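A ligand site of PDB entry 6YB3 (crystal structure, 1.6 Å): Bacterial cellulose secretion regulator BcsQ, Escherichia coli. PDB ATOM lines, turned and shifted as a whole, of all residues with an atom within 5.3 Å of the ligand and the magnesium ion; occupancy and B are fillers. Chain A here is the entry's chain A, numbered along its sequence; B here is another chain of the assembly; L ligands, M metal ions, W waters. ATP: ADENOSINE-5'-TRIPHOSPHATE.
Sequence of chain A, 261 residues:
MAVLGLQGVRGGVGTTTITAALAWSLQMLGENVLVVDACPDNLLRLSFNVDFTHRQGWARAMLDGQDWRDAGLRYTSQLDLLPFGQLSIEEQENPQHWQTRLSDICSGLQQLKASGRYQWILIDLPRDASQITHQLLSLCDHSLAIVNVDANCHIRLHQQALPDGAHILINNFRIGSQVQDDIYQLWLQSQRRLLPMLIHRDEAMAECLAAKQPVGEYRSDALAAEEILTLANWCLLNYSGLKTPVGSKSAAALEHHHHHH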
ATOM      1  N   ARG A  10     -35.106   9.838 -31.442  1.00  0.00           N
ATOM      2  CA  ARG A  10     -35.584   9.310 -30.184  1.00  0.00           C
ATOM      3  C   ARG A  10     -35.593  10.465 -29.198  1.00  0.00           C
ATOM      4  O   ARG A  10     -34.919  11.479 -29.407  1.00  0.00           O
ATOM      5  CB  ARG A  10     -34.668   8.164 -29.733  1.00  0.00           C
ATOM      6  CG  ARG A  10     -34.767   7.763 -28.287  1.00  0.00           C
ATOM      7  CD  ARG A  10     -33.708   6.770 -28.038  1.00  0.00           C
ATOM      8  NE  ARG A  10     -32.459   7.362 -27.559  1.00  0.00           N
ATOM      9  CZ  ARG A  10     -31.263   6.859 -27.852  1.00  0.00           C
ATOM     10  NH1 ARG A  10     -31.174   5.823 -28.674  1.00  0.00           N
ATOM     11  NH2 ARG A  10     -30.156   7.413 -27.363  1.00  0.00           N
ATOM     12  N   GLY A  11     -36.333  10.306 -28.100  1.00  0.00           N
ATOM     13  CA  GLY A  11     -36.247  11.278 -27.031  1.00  0.00           C
ATOM     14  C   GLY A  11     -34.863  11.307 -26.408  1.00  0.00           C
ATOM     15  O   GLY A  11     -34.120  10.325 -26.446  1.00  0.00           O
ATOM     16  N   GLY A  12     -34.499  12.457 -25.852  1.00  0.00           N
ATOM     17  CA  GLY A  12     -33.312  12.534 -25.015  1.00  0.00           C
ATOM     18  C   GLY A  12     -31.981  12.586 -25.731  1.00  0.00           C
ATOM     19  O   GLY A  12     -30.936  12.493 -25.063  1.00  0.00           O
ATOM     20  N   VAL A  13     -31.952  12.743 -27.057  1.00  0.00           N
ATOM     21  CA  VAL A  13     -30.702  12.698 -27.788  1.00  0.00           C
ATOM     22  C   VAL A  13     -29.981  14.043 -27.860  1.00  0.00           C
ATOM     23  O   VAL A  13     -28.861  14.074 -28.392  1.00  0.00           O
ATOM     24  CB  VAL A  13     -30.887  12.178 -29.226  1.00  0.00           C
ATOM     25  CG1 VAL A  13     -31.307  10.709 -29.177  1.00  0.00           C
ATOM     26  CG2 VAL A  13     -31.939  13.022 -29.973  1.00  0.00           C
ATOM     27  N   GLY A  14     -30.576  15.135 -27.371  1.00  0.00           N
ATOM     28  CA  GLY A  14     -29.890  16.431 -27.345  1.00  0.00           C
ATOM     29  C   GLY A  14     -30.559  17.538 -28.147  1.00  0.00           C
ATOM     30  O   GLY A  14     -29.983  18.613 -28.325  1.00  0.00           O
ATOM     31  N   THR A  15     -31.800  17.293 -28.593  1.00  0.00           N
ATOM     32  CA  THR A  15     -32.415  18.161 -29.596  1.00  0.00           C
ATOM     33  C   THR A  15     -32.589  19.581 -29.070  1.00  0.00           C
ATOM     34  O   THR A  15     -32.299  20.549 -29.781  1.00  0.00           O
ATOM     35  CB  THR A  15     -33.773  17.566 -30.003  1.00  0.00           C
ATOM     36  OG1 THR A  15     -33.553  16.238 -30.457  1.00  0.00           O
ATOM     37  CG2 THR A  15     -34.398  18.407 -31.137  1.00  0.00           C
ATOM     38  N   THR A  16     -33.076  19.725 -27.848  1.00  0.00           N
ATOM     39  CA  THR A  16     -33.353  21.060 -27.309  1.00  0.00           C
ATOM     40  C   THR A  16     -32.058  21.829 -27.030  1.00  0.00           C
ATOM     41  O   THR A  16     -31.945  23.024 -27.339  1.00  0.00           O
ATOM     42  CB  THR A  16     -34.200  20.906 -26.049  1.00  0.00           C
ATOM     43  OG1 THR A  16     -35.453  20.308 -26.428  1.00  0.00           O
ATOM     44  CG2 THR A  16     -34.494  22.282 -25.452  1.00  0.00           C
ATOM     45  N   THR A  17     -31.070  21.146 -26.443  1.00  0.00           N
ATOM     46  CA  THR A  17     -29.795  21.819 -26.194  1.00  0.00           C
ATOM     47  C   THR A  17     -29.143  22.261 -27.506  1.00  0.00           C
ATOM     48  O   THR A  17     -28.609  23.375 -27.599  1.00  0.00           O
ATOM     49  CB  THR A  17     -28.868  20.904 -25.396  1.00  0.00           C
ATOM     50  OG1 THR A  17     -29.522  20.499 -24.206  1.00  0.00           O
ATOM     51  CG2 THR A  17     -27.565  21.650 -25.016  1.00  0.00           C
ATOM     52  N   ILE A  18     -29.235  21.428 -28.539  1.00  0.00           N
ATOM     53  CA  ILE A  18     -28.694  21.803 -29.848  1.00  0.00           C
ATOM     54  C   ILE A  18     -29.485  22.954 -30.470  1.00  0.00           C
ATOM     55  O   ILE A  18     -28.898  23.850 -31.105  1.00  0.00           O
ATOM     56  CB  ILE A  18     -28.671  20.579 -30.782  1.00  0.00           C
ATOM     57  CG1 ILE A  18     -27.629  19.569 -30.293  1.00  0.00           C
ATOM     58  CG2 ILE A  18     -28.368  21.010 -32.222  1.00  0.00           C
ATOM     59  CD1 ILE A  18     -27.735  18.225 -30.994  1.00  0.00           C
ATOM     60  N   CYS A  39     -42.427  21.682 -28.219  1.00  0.00           N
ATOM     61  CA  CYS A  39     -42.530  20.523 -27.338  1.00  0.00           C
ATOM     62  C   CYS A  39     -43.385  20.830 -26.129  1.00  0.00           C
ATOM     63  O   CYS A  39     -43.118  21.815 -25.428  1.00  0.00           O
ATOM     64  CB  CYS A  39     -41.146  20.107 -26.855  1.00  0.00           C
ATOM     65  SG  CYS A  39     -40.040  19.688 -28.161  1.00  0.00           S
ATOM     66  N   ASP A  41     -43.313  19.685 -23.258  1.00  0.00           N
ATOM     67  CA  ASP A  41     -42.534  19.753 -22.022  1.00  0.00           C
ATOM     68  C   ASP A  41     -41.956  21.141 -21.766  1.00  0.00           C
ATOM     69  O   ASP A  41     -41.460  21.380 -20.657  1.00  0.00           O
ATOM     70  CB  ASP A  41     -41.419  18.717 -22.049  1.00  0.00           C
ATOM     71  CG  ASP A  41     -40.642  18.743 -23.351  1.00  0.00           C
ATOM     72  OD1 ASP A  41     -41.059  18.070 -24.313  1.00  0.00           O
ATOM     73  OD2 ASP A  41     -39.621  19.462 -23.425  1.00  0.00           O
ATOM     74  N   LEU A  43     -39.285  22.905 -22.352  1.00  0.00           N
ATOM     75  CA  LEU A  43     -37.951  22.982 -21.764  1.00  0.00           C
ATOM     76  C   LEU A  43     -37.049  24.034 -22.397  1.00  0.00           C
ATOM     77  O   LEU A  43     -36.140  24.528 -21.722  1.00  0.00           O
ATOM     78  CB  LEU A  43     -37.245  21.624 -21.846  1.00  0.00           C
ATOM     79  CG  LEU A  43     -37.951  20.502 -21.065  1.00  0.00           C
ATOM     80  CD1 LEU A  43     -37.284  19.146 -21.272  1.00  0.00           C
ATOM     81  CD2 LEU A  43     -38.012  20.863 -19.593  1.00  0.00           C
ATOM     82  N   ASP A 124     -37.951  23.636 -32.245  1.00  0.00           N
ATOM     83  CA  ASP A 124     -37.654  22.431 -31.471  1.00  0.00           C
ATOM     84  C   ASP A 124     -38.890  21.538 -31.521  1.00  0.00           C
ATOM     85  O   ASP A 124     -39.920  21.871 -30.920  1.00  0.00           O
ATOM     86  CB  ASP A 124     -37.274  22.845 -30.055  1.00  0.00           C
ATOM     87  CG  ASP A 124     -36.911  21.689 -29.157  1.00  0.00           C
ATOM     88  OD1 ASP A 124     -36.908  20.522 -29.592  1.00  0.00           O
ATOM     89  OD2 ASP A 124     -36.633  21.988 -27.977  1.00  0.00           O
ATOM     90  N   ASN A 171     -24.988  13.527 -32.161  1.00  0.00           N
ATOM     91  CA  ASN A 171     -24.681  14.235 -30.927  1.00  0.00           C
ATOM     92  C   ASN A 171     -24.208  13.213 -29.903  1.00  0.00           C
ATOM     93  O   ASN A 171     -24.413  12.010 -30.073  1.00  0.00           O
ATOM     94  CB  ASN A 171     -25.917  15.011 -30.413  1.00  0.00           C
ATOM     95  CG  ASN A 171     -25.647  15.793 -29.134  1.00  0.00           C
ATOM     96  OD1 ASN A 171     -24.621  16.460 -28.996  1.00  0.00           O
ATOM     97  ND2 ASN A 171     -26.569  15.700 -28.193  1.00  0.00           N
ATOM     98  N   ASN A 172     -23.541  13.715 -28.856  1.00  0.00           N
ATOM     99  CA  ASN A 172     -23.121  12.903 -27.720  1.00  0.00           C
ATOM    100  C   ASN A 172     -22.054  11.871 -28.102  1.00  0.00           C
ATOM    101  O   ASN A 172     -21.943  10.812 -27.467  1.00  0.00           O
ATOM    102  CB  ASN A 172     -24.307  12.197 -27.058  1.00  0.00           C
ATOM    103  CG  ASN A 172     -24.871  12.971 -25.876  1.00  0.00           C
ATOM    104  OD1 ASN A 172     -24.126  13.527 -25.076  1.00  0.00           O
ATOM    105  ND2 ASN A 172     -26.195  12.974 -25.763  1.00  0.00           N
ATOM    106  N   ILE A 199     -21.330  16.433 -33.004  1.00  0.00           N
ATOM    107  CA  ILE A 199     -21.201  17.118 -31.724  1.00  0.00           C
ATOM    108  C   ILE A 199     -20.745  16.086 -30.700  1.00  0.00           C
ATOM    109  O   ILE A 199     -21.437  15.098 -30.453  1.00  0.00           O
ATOM    110  CB  ILE A 199     -22.528  17.763 -31.284  1.00  0.00           C
ATOM    111  CG1 ILE A 199     -23.185  18.524 -32.438  1.00  0.00           C
ATOM    112  CG2 ILE A 199     -22.312  18.660 -30.073  1.00  0.00           C
ATOM    113  CD1 ILE A 199     -22.293  19.593 -33.073  1.00  0.00           C
ATOM    114  N   HIS A 200     -19.566  16.302 -30.118  1.00  0.00           N
ATOM    115  CA  HIS A 200     -19.048  15.364 -29.132  1.00  0.00           C
ATOM    116  C   HIS A 200     -19.781  15.495 -27.799  1.00  0.00           C
ATOM    117  O   HIS A 200     -20.299  16.554 -27.443  1.00  0.00           O
ATOM    118  CB  HIS A 200     -17.553  15.619 -28.896  1.00  0.00           C
ATOM    119  CG  HIS A 200     -16.662  14.984 -29.923  1.00  0.00           C
ATOM    120  ND1 HIS A 200     -16.377  15.573 -31.128  1.00  0.00           N
ATOM    121  CD2 HIS A 200     -15.993  13.809 -29.903  1.00  0.00           C
ATOM    122  CE1 HIS A 200     -15.567  14.784 -31.827  1.00  0.00           C
ATOM    123  NE2 HIS A 200     -15.322  13.708 -31.100  1.00  0.00           N
ATOM    124  N   ARG A 201     -19.815  14.392 -27.044  1.00  0.00           N
ATOM    125  CA  ARG A 201     -20.136  14.511 -25.628  1.00  0.00           C
ATOM    126  C   ARG A 201     -19.211  15.561 -25.005  1.00  0.00           C
ATOM    127  O   ARG A 201     -17.994  15.533 -25.217  1.00  0.00           O
ATOM    128  CB  ARG A 201     -19.993  13.160 -24.913  1.00  0.00           C
ATOM    129  CG  ARG A 201     -19.729  13.275 -23.419  1.00  0.00           C
ATOM    130  CD  ARG A 201     -20.473  12.214 -22.623  1.00  0.00           C
ATOM    131  NE  ARG A 201     -21.819  12.674 -22.311  1.00  0.00           N
ATOM    132  CZ  ARG A 201     -22.788  11.900 -21.820  1.00  0.00           C
ATOM    133  NH1 ARG A 201     -22.566  10.609 -21.592  1.00  0.00           N
ATOM    134  NH2 ARG A 201     -23.978  12.438 -21.567  1.00  0.00           N
ATOM    135  N   ASP A 202     -19.799  16.521 -24.281  1.00  0.00           N
ATOM    136  CA  ASP A 202     -19.030  17.624 -23.732  1.00  0.00           C
ATOM    137  C   ASP A 202     -19.713  18.063 -22.453  1.00  0.00           C
ATOM    138  O   ASP A 202     -20.936  18.259 -22.456  1.00  0.00           O
ATOM    139  CB  ASP A 202     -18.947  18.772 -24.755  1.00  0.00           C
ATOM    140  CG  ASP A 202     -17.974  19.883 -24.350  1.00  0.00           C
ATOM    141  OD1 ASP A 202     -17.888  20.243 -23.157  1.00  0.00           O
ATOM    142  OD2 ASP A 202     -17.318  20.426 -25.262  1.00  0.00           O
ATOM    143  N   GLU A 203     -18.970  18.183 -21.341  1.00  0.00           N
ATOM    144  CA  GLU A 203     -19.620  18.593 -20.099  1.00  0.00           C
ATOM    145  C   GLU A 203     -20.212  19.996 -20.198  1.00  0.00           C
ATOM    146  O   GLU A 203     -21.105  20.332 -19.405  1.00  0.00           O
ATOM    147  CB  GLU A 203     -18.663  18.509 -18.905  1.00  0.00           C
ATOM    148  CG  GLU A 203     -18.405  17.093 -18.441  1.00  0.00           C
ATOM    149  CD  GLU A 203     -19.686  16.344 -18.066  1.00  0.00           C
ATOM    150  OE1 GLU A 203     -20.470  16.843 -17.228  1.00  0.00           O
ATOM    151  OE2 GLU A 203     -19.898  15.251 -18.611  1.00  0.00           O
ATOM    152  N   MET A 205     -22.116  20.948 -22.532  1.00  0.00           N
ATOM    153  CA  MET A 205     -23.495  20.679 -22.959  1.00  0.00           C
ATOM    154  C   MET A 205     -24.340  20.131 -21.821  1.00  0.00           C
ATOM    155  O   MET A 205     -25.572  20.249 -21.853  1.00  0.00           O
ATOM    156  CB  MET A 205     -23.510  19.697 -24.122  1.00  0.00           C
ATOM    157  CG  MET A 205     -22.868  20.192 -25.416  1.00  0.00           C
ATOM    158  SD  MET A 205     -23.966  21.250 -26.382  1.00  0.00           S
ATOM    159  CE  MET A 205     -25.071  20.025 -27.096  1.00  0.00           C
ATOM    160  N   ALA A 206     -23.721  19.452 -20.842  1.00  0.00           N
ATOM    161  CA  ALA A 206     -24.484  19.015 -19.669  1.00  0.00           C
ATOM    162  C   ALA A 206     -24.681  20.150 -18.677  1.00  0.00           C
ATOM    163  O   ALA A 206     -25.734  20.227 -18.022  1.00  0.00           O
ATOM    164  CB  ALA A 206     -23.786  17.835 -18.984  1.00  0.00           C
ATOM    165  N   GLU A 207     -23.703  21.055 -18.568  1.00  0.00           N
ATOM    166  CA  GLU A 207     -23.749  22.139 -17.603  1.00  0.00           C
ATOM    167  C   GLU A 207     -24.600  23.313 -18.060  1.00  0.00           C
ATOM    168  O   GLU A 207     -25.172  24.022 -17.219  1.00  0.00           O
ATOM    169  CB  GLU A 207     -22.337  22.640 -17.319  1.00  0.00           C
ATOM    170  CG  GLU A 207     -21.496  21.585 -16.585  1.00  0.00           C
ATOM    171  CD  GLU A 207     -20.039  21.973 -16.466  1.00  0.00           C
ATOM    172  OE1 GLU A 207     -19.657  23.072 -16.941  1.00  0.00           O
ATOM    173  OE2 GLU A 207     -19.272  21.191 -15.884  1.00  0.00           O
ATOM    174  N   LEU A 209     -27.440  23.906 -19.437  1.00  0.00           N
ATOM    175  CA  LEU A 209     -28.839  23.979 -19.011  1.00  0.00           C
ATOM    176  C   LEU A 209     -28.933  24.276 -17.520  1.00  0.00           C
ATOM    177  O   LEU A 209     -29.807  25.043 -17.076  1.00  0.00           O
ATOM    178  CB  LEU A 209     -29.573  22.680 -19.342  1.00  0.00           C
ATOM    179  CG  LEU A 209     -31.050  22.619 -18.978  1.00  0.00           C
ATOM    180  CD1 LEU A 209     -31.774  23.863 -19.527  1.00  0.00           C
ATOM    181  CD2 LEU A 209     -31.721  21.332 -19.495  1.00  0.00           C
ATOM    182  N   ARG B  10     -38.329  10.497 -19.515  1.00  0.00           N
ATOM    183  CA  ARG B  10     -38.239  10.981 -20.884  1.00  0.00           C
ATOM    184  C   ARG B  10     -37.737   9.830 -21.740  1.00  0.00           C
ATOM    185  O   ARG B  10     -37.334   8.787 -21.232  1.00  0.00           O
ATOM    186  CB  ARG B  10     -37.329  12.214 -21.008  1.00  0.00           C
ATOM    187  CG  ARG B  10     -35.878  11.927 -20.784  1.00  0.00           C
ATOM    188  CD  ARG B  10     -34.936  12.786 -21.650  1.00  0.00           C
ATOM    189  NE  ARG B  10     -33.596  12.234 -21.559  1.00  0.00           N
ATOM    190  CZ  ARG B  10     -32.682  12.640 -20.682  1.00  0.00           C
ATOM    191  NH1 ARG B  10     -32.971  13.615 -19.834  1.00  0.00           N
ATOM    192  NH2 ARG B  10     -31.492  12.052 -20.642  1.00  0.00           N
ATOM    193  N   GLY B  11     -37.783  10.012 -23.063  1.00  0.00           N
ATOM    194  CA  GLY B  11     -37.292   8.980 -23.953  1.00  0.00           C
ATOM    195  C   GLY B  11     -35.799   8.748 -23.797  1.00  0.00           C
ATOM    196  O   GLY B  11     -35.047   9.621 -23.364  1.00  0.00           O
ATOM    197  N   ASP B 150     -29.503  14.203 -14.960  1.00  0.00           N
ATOM    198  CA  ASP B 150     -29.123  15.360 -15.758  1.00  0.00           C
ATOM    199  C   ASP B 150     -30.160  16.458 -15.536  1.00  0.00           C
ATOM    200  O   ASP B 150     -31.163  16.275 -14.840  1.00  0.00           O
ATOM    201  CB  ASP B 150     -28.949  15.008 -17.241  1.00  0.00           C
ATOM    202  CG  ASP B 150     -30.189  14.399 -17.880  1.00  0.00           C
ATOM    203  OD1 ASP B 150     -31.320  14.900 -17.662  1.00  0.00           O
ATOM    204  OD2 ASP B 150     -30.028  13.433 -18.658  1.00  0.00           O
ATOM    205  N   ALA B 151     -29.890  17.635 -16.112  1.00  0.00           N
ATOM    206  CA  ALA B 151     -30.731  18.787 -15.805  1.00  0.00           C
ATOM    207  C   ALA B 151     -32.120  18.629 -16.406  1.00  0.00           C
ATOM    208  O   ALA B 151     -33.098  19.109 -15.824  1.00  0.00           O
ATOM    209  CB  ALA B 151     -30.076  20.074 -16.303  1.00  0.00           C
ATOM    210  N   ASN B 152     -32.233  17.940 -17.544  1.00  0.00           N
ATOM    211  CA  ASN B 152     -33.516  17.669 -18.163  1.00  0.00           C
ATOM    212  C   ASN B 152     -34.413  16.827 -17.254  1.00  0.00           C
ATOM    213  O   ASN B 152     -35.545  17.206 -16.952  1.00  0.00           O
ATOM    214  CB  ASN B 152     -33.258  17.012 -19.532  1.00  0.00           C
ATOM    215  CG  ASN B 152     -34.519  16.503 -20.235  1.00  0.00           C
ATOM    216  OD1 ASN B 152     -35.366  15.844 -19.647  1.00  0.00           O
ATOM    217  ND2 ASN B 152     -34.581  16.747 -21.540  1.00  0.00           N
ATOM    218  N   ARG B 156     -37.931  17.829 -15.223  1.00  0.00           N
ATOM    219  CA  ARG B 156     -39.143  17.053 -15.474  1.00  0.00           C
ATOM    220  C   ARG B 156     -39.770  16.591 -14.170  1.00  0.00           C
ATOM    221  O   ARG B 156     -40.990  16.576 -14.038  1.00  0.00           O
ATOM    222  CB  ARG B 156     -38.840  15.870 -16.396  1.00  0.00           C
ATOM    223  CG  ARG B 156     -38.642  16.247 -17.874  1.00  0.00           C
ATOM    224  CD  ARG B 156     -38.279  15.014 -18.700  1.00  0.00           C
ATOM    225  NE  ARG B 156     -38.217  15.301 -20.126  1.00  0.00           N
ATOM    226  CZ  ARG B 156     -39.259  15.232 -20.942  1.00  0.00           C
ATOM    227  NH1 ARG B 156     -40.448  14.861 -20.478  1.00  0.00           N
ATOM    228  NH2 ARG B 156     -39.135  15.518 -22.243  1.00  0.00           N
ATOM    229  N   ARG B 174     -22.513   8.105 -14.657  1.00  0.00           N
ATOM    230  CA  ARG B 174     -21.168   8.001 -15.208  1.00  0.00           C
ATOM    231  C   ARG B 174     -20.135   8.735 -14.368  1.00  0.00           C
ATOM    232  O   ARG B 174     -20.448   9.512 -13.458  1.00  0.00           O
ATOM    233  CB  ARG B 174     -21.112   8.530 -16.651  1.00  0.00           C
ATOM    234  CG  ARG B 174     -21.602   9.929 -16.842  1.00  0.00           C
ATOM    235  CD  ARG B 174     -21.595  10.236 -18.334  1.00  0.00           C
ATOM    236  NE  ARG B 174     -22.161  11.545 -18.660  1.00  0.00           N
ATOM    237  CZ  ARG B 174     -21.488  12.684 -18.591  1.00  0.00           C
ATOM    238  NH1 ARG B 174     -20.223  12.683 -18.198  1.00  0.00           N
ATOM    239  NH2 ARG B 174     -22.087  13.833 -18.907  1.00  0.00           N
HETATM  240  PG  ATP L   1     -36.296  15.518 -24.662  1.00  0.00           P
HETATM  241  O1G ATP L   1     -36.720  15.575 -23.233  1.00  0.00           O
HETATM  242  O2G ATP L   1     -36.682  14.213 -25.397  1.00  0.00           O
HETATM  243  O3G ATP L   1     -36.920  16.614 -25.520  1.00  0.00           O
HETATM  244  PB  ATP L   1     -33.775  16.254 -25.900  1.00  0.00           P
HETATM  245  O1B ATP L   1     -33.540  15.277 -26.982  1.00  0.00           O
HETATM  246  O2B ATP L   1     -34.303  17.641 -26.285  1.00  0.00           O
HETATM  247  O3B ATP L   1     -34.714  15.686 -24.759  1.00  0.00           O
HETATM  248  PA  ATP L   1     -31.868  17.672 -24.201  1.00  0.00           P
HETATM  249  O1A ATP L   1     -32.836  18.187 -23.218  1.00  0.00           O
HETATM  250  O2A ATP L   1     -31.271  18.630 -25.208  1.00  0.00           O
HETATM  251  O3A ATP L   1     -32.446  16.464 -25.054  1.00  0.00           O
HETATM  252  O5' ATP L   1     -30.624  16.941 -23.502  1.00  0.00           O
HETATM  253  C5' ATP L   1     -30.849  15.878 -22.543  1.00  0.00           C
HETATM  254  C4' ATP L   1     -29.713  15.946 -21.549  1.00  0.00           C
HETATM  255  O4' ATP L   1     -28.493  15.538 -22.204  1.00  0.00           O
HETATM  256  C3' ATP L   1     -29.476  17.338 -20.969  1.00  0.00           C
HETATM  257  O3' ATP L   1     -29.390  17.329 -19.547  1.00  0.00           O
HETATM  258  C2' ATP L   1     -28.204  17.813 -21.670  1.00  0.00           C
HETATM  259  O2' ATP L   1     -27.491  18.704 -20.819  1.00  0.00           O
HETATM  260  C1' ATP L   1     -27.475  16.499 -21.982  1.00  0.00           C
HETATM  261  N9  ATP L   1     -26.655  16.557 -23.192  1.00  0.00           N
HETATM  262  C8  ATP L   1     -27.125  16.814 -24.460  1.00  0.00           C
HETATM  263  N7  ATP L   1     -26.198  16.876 -25.380  1.00  0.00           N
HETATM  264  C5  ATP L   1     -25.026  16.629 -24.677  1.00  0.00           C
HETATM  265  C6  ATP L   1     -23.682  16.548 -25.078  1.00  0.00           C
HETATM  266  N6  ATP L   1     -23.272  16.670 -26.352  1.00  0.00           N
HETATM  267  N1  ATP L   1     -22.747  16.316 -24.124  1.00  0.00           N
HETATM  268  C2  ATP L   1     -23.158  16.158 -22.859  1.00  0.00           C
HETATM  269  N3  ATP L   1     -24.396  16.169 -22.368  1.00  0.00           N
HETATM  270  C4  ATP L   1     -25.295  16.422 -23.330  1.00  0.00           C
HETATM  271 MG    MG M   1     -36.134  18.430 -25.949  1.00  0.00          MG
HETATM  272  O   HOH W   1     -35.493  18.833 -23.949  1.00  0.00           O
HETATM  273  O   HOH W   2     -32.277  21.239 -23.111  1.00  0.00           O
HETATM  274  O   HOH W   3     -37.940  19.323 -25.353  1.00  0.00           O
HETATM  275  O   HOH W   4     -27.290  17.944 -17.434  1.00  0.00           O
HETATM  276  O   HOH W   5     -36.779  18.298 -27.895  1.00  0.00           O
HETATM  277  O   HOH W   6     -37.743  15.039 -27.950  1.00  0.00           O
HETATM  278  O   HOH W   7     -38.446  12.389 -24.495  1.00  0.00           O
HETATM  279  O   HOH W   8     -35.234  14.447 -28.817  1.00  0.00           O
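An oxygen (O2A) of the ligand sits at hydrogen-bond distance from the backbone NH (N) of Thr 16, 3.4 Å away.
The guanidinium group (NH2) of Arg 156 of chain B is in salt-bridge range of an oxygen (O1G) of the ligand, 2.6 Å away.
O of Met 205 sits at hydrogen-bond distance from O2' of the ligand, at 2.7 Å.
The backbone NH (N) of Thr 17 sits at hydrogen-bond distance from an oxygen (O2A) of the ligand (2.8 Å).
An oxygen (O2A) of the ligand lies within hydrogen-bond range of the side-chain hydroxyl of Thr 17, at 2.7 Å.
ND2 of Asn 152 of chain B lies within hydrogen-bond range of O1A of the ligand, at 2.8 Å.
The backbone NH (N) of Gly 12 sits at hydrogen-bond distance from an oxygen (O2G) of the ligand.
The backbone NH (N) of Asp 202 is in hydrogen-bond range of a nitrogen (N1) of the ligand (3.0 Å).
The side-chain amide oxygen of Asn 171 lies within hydrogen-bond range of a nitrogen (N6) of the ligand (3.0 Å).
The backbone NH (N) of Val 13 sits at hydrogen-bond distance from an oxygen (O1B) of the ligand, at 3.0 Å.
An oxygen (O1B) of the ligand lies within hydrogen-bond range of the backbone NH (N) of Gly 14, 3.0 Å away.
The side-chain amide oxygen (OD1) of Asn 172 sits close to a nitrogen (N1) of the ligand, 3.3 Å away.
The backbone NH (N) of Thr 15 lies within hydrogen-bond range of an oxygen (O1B) of the ligand (3.1 Å).
The backbone carbonyl oxygen (O) of His 200 sits at hydrogen-bond distance from a nitrogen (N6) of the ligand, at 3.2 Å.
O3' of the ligand lies within hydrogen-bond range of N of Ala 151 of chain B.
OG1 of Thr 16 lies close to OD2 of Asp 124.
The side-chain amide oxygen (OD1) of Asn 152 of chain B lies within hydrogen-bond range of the guanidinium group (NE) of Arg 156 of chain B.
The guanidinium group (NH2) of Arg 156 of chain B is in salt-bridge range of the side-chain carboxylate (OD1) of Asp 41, 3.8 Å away.
The side-chain carboxylate (OD1) of Asp 150 of chain B lies within hydrogen-bond range of the backbone NH (N) of Asn 152 of chain B (3.2 Å).
The side-chain amide oxygen of Asn 152 of chain B sits at hydrogen-bond distance from the guanidinium group of Arg 10 of chain B, 3.3 Å away.
The side-chain amide nitrogen of Asn 171 sits at hydrogen-bond distance from the backbone carbonyl oxygen of Val 13 (2.8 Å).
N of Asn 172 is in hydrogen-bond range of O of Ile 199 (3.0 Å).
The guanidinium group of Arg 10 of chain B is in salt-bridge range of the side-chain carboxylate of Asp 150 of chain B (2.8 Å).
Residues that only touch the ligand: Ala 206 (3.2 Å), Asp 150 of chain B (3.3 Å), Gly 11 of chain A (3.4 Å), Arg 201 (3.5 Å) and Arg 10 of chain B (3.7 Å).
Within 4 Å of the ligand: Gly 11 of chain A, Gly 12, Val 13, Gly 14, Thr 15, Thr 16, Thr 17, Asn 171, Asn 172, His 200, Arg 201, Asp 202, Met 205, Ala 206, Arg 10 of chain B, Asp 150 of chain B, Ala 151 of chain B, Asn 152 of chain B and Arg 156 of chain B.
The nearest printed residue that does not touch the ligand is Leu 43 (4.1 Å).
The nearest printed residue that does not touch the magnesium ion is Asp 124 (4.1 Å).
The magnesium ion is bound by O2B of the ligand (2.0 Å), O3G of the ligand (2.0 Å), OG1 of Thr 16 (2.1 Å), water W5 (2.1 Å), water W3 (2.1 Å) and water W1 (2.1 Å).
Water W1 lies within hydrogen-bond range of an oxygen (O1A) of the ligand (2.8 Å) and the side-chain amide nitrogen (ND2) of Asn 152 of chain B (3.3 Å).
Water W3 lies within hydrogen-bond range of the side-chain carboxylate of Asp 41 (2.6 Å) and the side-chain sulfur of Cys 39 (3.5 Å).
Water W5 bridges the side-chain carboxylate of Asp 124 (2.8 Å) and the side-chain sulfur of Cys 39 (3.6 Å).
Water W8 lies within hydrogen-bond range of O1B of the ligand (2.6 Å), OG1 of Thr 15 (3.0 Å) and O of Arg 10 of chain A (3.0 Å).
Water W4 lies within hydrogen-bond range of O of Ala 206 (2.8 Å), N of Ala 151 of chain B (2.9 Å) and O3' of the ligand (3.0 Å).
Water W2 lies within hydrogen-bond range of OG1 of Thr 17 and O1A of the ligand.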
